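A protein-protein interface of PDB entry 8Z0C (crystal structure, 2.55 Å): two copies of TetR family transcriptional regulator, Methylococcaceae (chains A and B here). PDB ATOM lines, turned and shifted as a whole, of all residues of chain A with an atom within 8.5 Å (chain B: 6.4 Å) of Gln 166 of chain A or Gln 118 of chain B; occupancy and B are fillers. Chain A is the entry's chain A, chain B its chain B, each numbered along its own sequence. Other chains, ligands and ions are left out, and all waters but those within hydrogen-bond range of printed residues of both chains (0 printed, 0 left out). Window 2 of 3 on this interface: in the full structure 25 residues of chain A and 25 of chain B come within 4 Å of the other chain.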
ATOM      1  N   ILE A 160      28.826  -3.870  11.107  1.00  0.00           N
ATOM      2  CA  ILE A 160      27.699  -4.795  11.184  1.00  0.00           C
ATOM      3  C   ILE A 160      27.095  -5.010   9.802  1.00  0.00           C
ATOM      4  O   ILE A 160      26.595  -6.103   9.492  1.00  0.00           O
ATOM      5  CB  ILE A 160      26.633  -4.302  12.194  1.00  0.00           C
ATOM      6  CG1 ILE A 160      27.270  -3.751  13.475  1.00  0.00           C
ATOM      7  CG2 ILE A 160      25.689  -5.426  12.588  1.00  0.00           C
ATOM      8  CD1 ILE A 160      27.994  -4.822  14.324  1.00  0.00           C
ATOM      9  N   LEU A 163      28.488  -7.922   7.637  1.00  0.00           N
ATOM     10  CA  LEU A 163      28.243  -9.317   7.953  1.00  0.00           C
ATOM     11  C   LEU A 163      27.211  -9.960   7.049  1.00  0.00           C
ATOM     12  O   LEU A 163      27.117 -11.189   7.030  1.00  0.00           O
ATOM     13  CB  LEU A 163      27.795  -9.437   9.410  1.00  0.00           C
ATOM     14  CG  LEU A 163      28.816  -8.850  10.374  1.00  0.00           C
ATOM     15  CD1 LEU A 163      28.284  -8.861  11.792  1.00  0.00           C
ATOM     16  CD2 LEU A 163      30.103  -9.662  10.278  1.00  0.00           C
ATOM     17  N   GLY A 164      26.445  -9.172   6.304  1.00  0.00           N
ATOM     18  CA  GLY A 164      25.246  -9.711   5.685  1.00  0.00           C
ATOM     19  C   GLY A 164      24.208 -10.176   6.689  1.00  0.00           C
ATOM     20  O   GLY A 164      23.609 -11.243   6.507  1.00  0.00           O
ATOM     21  N   LEU A 165      23.978  -9.405   7.748  1.00  0.00           N
ATOM     22  CA  LEU A 165      23.048  -9.852   8.777  1.00  0.00           C
ATOM     23  C   LEU A 165      21.611  -9.747   8.293  1.00  0.00           C
ATOM     24  O   LEU A 165      21.251  -8.830   7.553  1.00  0.00           O
ATOM     25  CB  LEU A 165      23.226  -9.050  10.066  1.00  0.00           C
ATOM     26  CG  LEU A 165      24.351  -9.678  10.888  1.00  0.00           C
ATOM     27  CD1 LEU A 165      24.634  -8.871  12.137  1.00  0.00           C
ATOM     28  CD2 LEU A 165      24.022 -11.127  11.218  1.00  0.00           C
ATOM     29  N   GLN A 166      20.789 -10.697   8.725  1.00  0.00           N
ATOM     30  CA  GLN A 166      19.406 -10.760   8.280  1.00  0.00           C
ATOM     31  C   GLN A 166      18.552  -9.794   9.094  1.00  0.00           C
ATOM     32  O   GLN A 166      18.643  -9.748  10.327  1.00  0.00           O
ATOM     33  CB  GLN A 166      18.874 -12.193   8.395  1.00  0.00           C
ATOM     34  CG  GLN A 166      17.352 -12.314   8.229  1.00  0.00           C
ATOM     35  CD  GLN A 166      16.886 -12.144   6.781  1.00  0.00           C
ATOM     36  OE1 GLN A 166      17.504 -12.665   5.844  1.00  0.00           O
ATOM     37  NE2 GLN A 166      15.797 -11.395   6.594  1.00  0.00           N
ATOM     38  N   GLY A 167      17.725  -9.017   8.400  1.00  0.00           N
ATOM     39  CA  GLY A 167      16.869  -8.069   9.077  1.00  0.00           C
ATOM     40  C   GLY A 167      17.544  -6.774   9.448  1.00  0.00           C
ATOM     41  O   GLY A 167      17.060  -6.060  10.339  1.00  0.00           O
ATOM     42  N   LEU A 168      18.655  -6.446   8.795  1.00  0.00           N
ATOM     43  CA  LEU A 168      19.336  -5.175   9.016  1.00  0.00           C
ATOM     44  C   LEU A 168      19.640  -4.602   7.636  1.00  0.00           C
ATOM     45  O   LEU A 168      20.554  -5.073   6.951  1.00  0.00           O
ATOM     46  CB  LEU A 168      20.589  -5.376   9.857  1.00  0.00           C
ATOM     47  CG  LEU A 168      21.600  -4.240   9.954  1.00  0.00           C
ATOM     48  CD1 LEU A 168      20.926  -2.944  10.446  1.00  0.00           C
ATOM     49  CD2 LEU A 168      22.735  -4.657  10.882  1.00  0.00           C
ATOM     50  N   ALA A 169      18.857  -3.603   7.228  1.00  0.00           N
ATOM     51  CA  ALA A 169      18.883  -3.067   5.873  1.00  0.00           C
ATOM     52  C   ALA A 169      19.848  -1.892   5.782  1.00  0.00           C
ATOM     53  O   ALA A 169      19.834  -0.999   6.636  1.00  0.00           O
ATOM     54  CB  ALA A 169      17.484  -2.626   5.437  1.00  0.00           C
ATOM     55  N   TYR B 113      28.826 -17.453  13.562  1.00  0.00           N
ATOM     56  CA  TYR B 113      28.972 -16.073  14.013  1.00  0.00           C
ATOM     57  C   TYR B 113      27.723 -15.257  13.710  1.00  0.00           C
ATOM     58  O   TYR B 113      27.283 -14.471  14.544  1.00  0.00           O
ATOM     59  CB  TYR B 113      30.199 -15.411  13.378  1.00  0.00           C
ATOM     60  CG  TYR B 113      30.501 -14.017  13.939  1.00  0.00           C
ATOM     61  CD1 TYR B 113      29.924 -12.874  13.391  1.00  0.00           C
ATOM     62  CD2 TYR B 113      31.361 -13.853  15.022  1.00  0.00           C
ATOM     63  CE1 TYR B 113      30.209 -11.611  13.902  1.00  0.00           C
ATOM     64  CE2 TYR B 113      31.650 -12.611  15.530  1.00  0.00           C
ATOM     65  CZ  TYR B 113      31.077 -11.492  14.970  1.00  0.00           C
ATOM     66  OH  TYR B 113      31.368 -10.253  15.515  1.00  0.00           O
ATOM     67  N   ASN B 114      27.126 -15.438  12.533  1.00  0.00           N
ATOM     68  CA  ASN B 114      25.911 -14.689  12.236  1.00  0.00           C
ATOM     69  C   ASN B 114      24.752 -15.136  13.118  1.00  0.00           C
ATOM     70  O   ASN B 114      24.006 -14.301  13.636  1.00  0.00           O
ATOM     71  CB  ASN B 114      25.556 -14.817  10.758  1.00  0.00           C
ATOM     72  CG  ASN B 114      26.216 -13.739   9.924  1.00  0.00           C
ATOM     73  OD1 ASN B 114      27.058 -12.993  10.430  1.00  0.00           O
ATOM     74  ND2 ASN B 114      25.836 -13.637   8.650  1.00  0.00           N
ATOM     75  N   LEU B 115      24.581 -16.447  13.301  1.00  0.00           N
ATOM     76  CA  LEU B 115      23.510 -16.928  14.161  1.00  0.00           C
ATOM     77  C   LEU B 115      23.647 -16.377  15.580  1.00  0.00           C
ATOM     78  O   LEU B 115      22.652 -15.995  16.204  1.00  0.00           O
ATOM     79  CB  LEU B 115      23.502 -18.458  14.176  1.00  0.00           C
ATOM     80  CG  LEU B 115      22.703 -19.148  13.071  1.00  0.00           C
ATOM     81  CD1 LEU B 115      23.379 -20.477  12.716  1.00  0.00           C
ATOM     82  CD2 LEU B 115      21.277 -19.395  13.502  1.00  0.00           C
ATOM     83  N   ALA B 116      24.874 -16.338  16.105  1.00  0.00           N
ATOM     84  CA  ALA B 116      25.073 -15.857  17.462  1.00  0.00           C
ATOM     85  C   ALA B 116      24.747 -14.371  17.564  1.00  0.00           C
ATOM     86  O   ALA B 116      24.060 -13.947  18.505  1.00  0.00           O
ATOM     87  CB  ALA B 116      26.505 -16.148  17.919  1.00  0.00           C
ATOM     88  N   MET B 117      25.205 -13.574  16.588  1.00  0.00           N
ATOM     89  CA  MET B 117      24.865 -12.150  16.549  1.00  0.00           C
ATOM     90  C   MET B 117      23.359 -11.939  16.430  1.00  0.00           C
ATOM     91  O   MET B 117      22.804 -11.008  17.028  1.00  0.00           O
ATOM     92  CB  MET B 117      25.590 -11.456  15.388  1.00  0.00           C
ATOM     93  CG  MET B 117      27.102 -11.280  15.578  1.00  0.00           C
ATOM     94  SD  MET B 117      27.549  -9.685  16.325  1.00  0.00           S
ATOM     95  CE  MET B 117      26.668  -8.570  15.254  1.00  0.00           C
ATOM     96  N   GLN B 118      22.673 -12.809  15.687  1.00  0.00           N
ATOM     97  CA  GLN B 118      21.231 -12.667  15.555  1.00  0.00           C
ATOM     98  C   GLN B 118      20.486 -13.038  16.835  1.00  0.00           C
ATOM     99  O   GLN B 118      19.439 -12.450  17.124  1.00  0.00           O
ATOM    100  CB  GLN B 118      20.729 -13.492  14.383  1.00  0.00           C
ATOM    101  CG  GLN B 118      20.583 -12.661  13.121  1.00  0.00           C
ATOM    102  CD  GLN B 118      20.485 -13.525  11.889  1.00  0.00           C
ATOM    103  OE1 GLN B 118      20.896 -13.123  10.792  1.00  0.00           O
ATOM    104  NE2 GLN B 118      19.951 -14.737  12.060  1.00  0.00           N
ATOM    105  N   SER B 119      20.992 -13.990  17.617  1.00  0.00           N
ATOM    106  CA  SER B 119      20.368 -14.229  18.913  1.00  0.00           C
ATOM    107  C   SER B 119      20.743 -13.156  19.942  1.00  0.00           C
ATOM    108  O   SER B 119      19.918 -12.818  20.805  1.00  0.00           O
ATOM    109  CB  SER B 119      20.747 -15.609  19.430  1.00  0.00           C
ATOM    110  OG  SER B 119      22.075 -15.584  19.901  1.00  0.00           O
ATOM    111  N   TRP B 120      21.977 -12.639  19.875  1.00  0.00           N
ATOM    112  CA  TRP B 120      22.373 -11.477  20.665  1.00  0.00           C
ATOM    113  C   TRP B 120      21.368 -10.342  20.508  1.00  0.00           C
ATOM    114  O   TRP B 120      20.911  -9.751  21.494  1.00  0.00           O
ATOM    115  CB  TRP B 120      23.761 -10.997  20.234  1.00  0.00           C
ATOM    116  CG  TRP B 120      24.369  -9.952  21.151  1.00  0.00           C
ATOM    117  CD1 TRP B 120      24.027  -9.708  22.453  1.00  0.00           C
ATOM    118  CD2 TRP B 120      25.420  -9.022  20.832  1.00  0.00           C
ATOM    119  NE1 TRP B 120      24.811  -8.706  22.964  1.00  0.00           N
ATOM    120  CE2 TRP B 120      25.674  -8.267  21.995  1.00  0.00           C
ATOM    121  CE3 TRP B 120      26.179  -8.763  19.681  1.00  0.00           C
ATOM    122  CZ2 TRP B 120      26.647  -7.257  22.040  1.00  0.00           C
ATOM    123  CZ3 TRP B 120      27.151  -7.765  19.729  1.00  0.00           C
ATOM    124  CH2 TRP B 120      27.373  -7.021  20.903  1.00  0.00           C
ATOM    125  N   HIS B 121      21.021 -10.033  19.256  1.00  0.00           N
ATOM    126  CA  HIS B 121      20.085  -8.960  18.956  1.00  0.00           C
ATOM    127  C   HIS B 121      18.707  -9.253  19.531  1.00  0.00           C
ATOM    128  O   HIS B 121      18.098  -8.391  20.166  1.00  0.00           O
ATOM    129  CB  HIS B 121      20.006  -8.778  17.446  1.00  0.00           C
ATOM    130  CG  HIS B 121      18.994  -7.767  17.010  1.00  0.00           C
ATOM    131  ND1 HIS B 121      17.695  -8.103  16.692  1.00  0.00           N
ATOM    132  CD2 HIS B 121      19.092  -6.427  16.835  1.00  0.00           C
ATOM    133  CE1 HIS B 121      17.040  -7.014  16.328  1.00  0.00           C
ATOM    134  NE2 HIS B 121      17.863  -5.984  16.410  1.00  0.00           N
ATOM    135  N   GLN B 122      18.192 -10.462  19.289  1.00  0.00           N
ATOM    136  CA  GLN B 122      16.938 -10.907  19.889  1.00  0.00           C
ATOM    137  C   GLN B 122      16.923 -10.631  21.384  1.00  0.00           C
ATOM    138  O   GLN B 122      15.974 -10.042  21.906  1.00  0.00           O
ATOM    139  CB  GLN B 122      16.732 -12.407  19.634  1.00  0.00           C
ATOM    140  CG  GLN B 122      15.884 -12.764  18.414  1.00  0.00           C
ATOM    141  CD  GLN B 122      16.288 -14.106  17.760  1.00  0.00           C
ATOM    142  OE1 GLN B 122      16.952 -14.958  18.378  1.00  0.00           O
ATOM    143  NE2 GLN B 122      15.911 -14.275  16.491  1.00  0.00           N
ATOM    144  N   ALA B 123      17.980 -11.041  22.085  1.00  0.00           N
ATOM    145  CA  ALA B 123      18.047 -10.835  23.526  1.00  0.00           C
ATOM    146  C   ALA B 123      17.979  -9.354  23.862  1.00  0.00           C
ATOM    147  O   ALA B 123      17.191  -8.935  24.716  1.00  0.00           O
ATOM    148  CB  ALA B 123      19.326 -11.454  24.093  1.00  0.00           C
ATOM    149  N   TRP B 148      19.779  -2.837  17.348  1.00  0.00           N
ATOM    150  CA  TRP B 148      20.865  -2.834  16.371  1.00  0.00           C
ATOM    151  C   TRP B 148      21.831  -1.691  16.628  1.00  0.00           C
ATOM    152  O   TRP B 148      23.049  -1.869  16.503  1.00  0.00           O
ATOM    153  CB  TRP B 148      20.323  -2.727  14.948  1.00  0.00           C
ATOM    154  CG  TRP B 148      19.779  -3.996  14.386  1.00  0.00           C
ATOM    155  CD1 TRP B 148      18.510  -4.209  13.931  1.00  0.00           C
ATOM    156  CD2 TRP B 148      20.486  -5.229  14.191  1.00  0.00           C
ATOM    157  NE1 TRP B 148      18.378  -5.492  13.471  1.00  0.00           N
ATOM    158  CE2 TRP B 148      19.579  -6.140  13.610  1.00  0.00           C
ATOM    159  CE3 TRP B 148      21.805  -5.647  14.434  1.00  0.00           C
ATOM    160  CZ2 TRP B 148      19.942  -7.451  13.279  1.00  0.00           C
ATOM    161  CZ3 TRP B 148      22.166  -6.958  14.100  1.00  0.00           C
ATOM    162  CH2 TRP B 148      21.234  -7.839  13.540  1.00  0.00           C
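The backbone carbonyl oxygen of Leu 163 of chain A sits at hydrogen-bond distance from the side-chain amide nitrogen of Asn 114 of chain B (3.2 Å).
The backbone NH of Gln 166 of chain A lies within hydrogen-bond range of the side-chain amide oxygen of Gln 118 of chain B.
The backbone carbonyl oxygen (O) of Gly 167 of chain A sits at hydrogen-bond distance from the indole nitrogen (NE1) of Trp 148 of chain B.
NE2 of His 121 of chain B is in hydrogen-bond range of NE1 of Trp 148 of chain B, 3.0 Å away.
CD1 of Leu 163 of chain A touches CE1 of Tyr 113 of chain B, at 3.96 Å.
Leu 163 of chain A touches Met 117 of chain B (CD1 to CE, 3.8 Å).
Asn 114 of chain B touches Gly 164 of chain A.
Leu 165 of chain A touches Asn 114 of chain B (CD2 to CG, 3.6 Å).
Met 117 of chain B touches Leu 165 of chain A (CE to CD1, 3.7 Å).
Gln 118 of chain B touches Leu 165 of chain A (OE1 to CD2, 3.7 Å).
CZ3 of Trp 148 of chain B touches CD1 of Leu 165 of chain A, 3.7 Å away.
Gln 166 of chain A touches Trp 148 of chain B.
CE3 of Trp 148 of chain B touches CD2 of Leu 168 of chain A (3.8 Å).
Of chain B, only Gln 118 (3.2 Å) and Trp 148 (3.96 Å) come within 4 Å of Gln 166 of chain A.
Of the printed residues of chain B, Leu 168 of chain A touches Trp 148.
Of the printed residues of chain A, Tyr 113 of chain B touches Leu 163.
Of the printed residues of chain A, Asn 114 of chain B touches Leu 163, Gly 164 and Leu 165.
Of the printed residues of chain A, Met 117 of chain B touches Leu 163 and Leu 165.
Of chain A, only Leu 165 and Gln 166 come within 4 Å of Gln 118 of chain B.
No residue of chain A comes within 4 Å of Ser 119 of chain B.
Of the printed residues of chain A, Trp 148 of chain B touches Leu 165 (3.7 Å), Gln 166 (3.96 Å), Gly 167 (3.4 Å) and Leu 168 (3.8 Å).
The nearest residue of chain A that does not touch Gln 118 of chain B is Gly 164 of chain A (5.4 Å).
The nearest printed residue of chain A that does not touch Met 117 of chain B is Ile 160 of chain A (4.1 Å).
Of the 12 printed residues of chain B, 5 touch a printed residue of chain A.
Hydrophobic or aromatic side chains of chain B within 4 Å of the printed part of chain A: Tyr 113, Met 117 and Trp 148.
Among the printed residues, 12 pairs touch across the chains.
Among the printed residues, no Asp or Glu carboxylate lies within 4 Å of a Lys or Arg side-chain nitrogen of the other chain.
No position is printed for both chains.
Of the 12 pairs that touch across the chains among the printed residues, none has its exchanged pair printed and touching as well.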
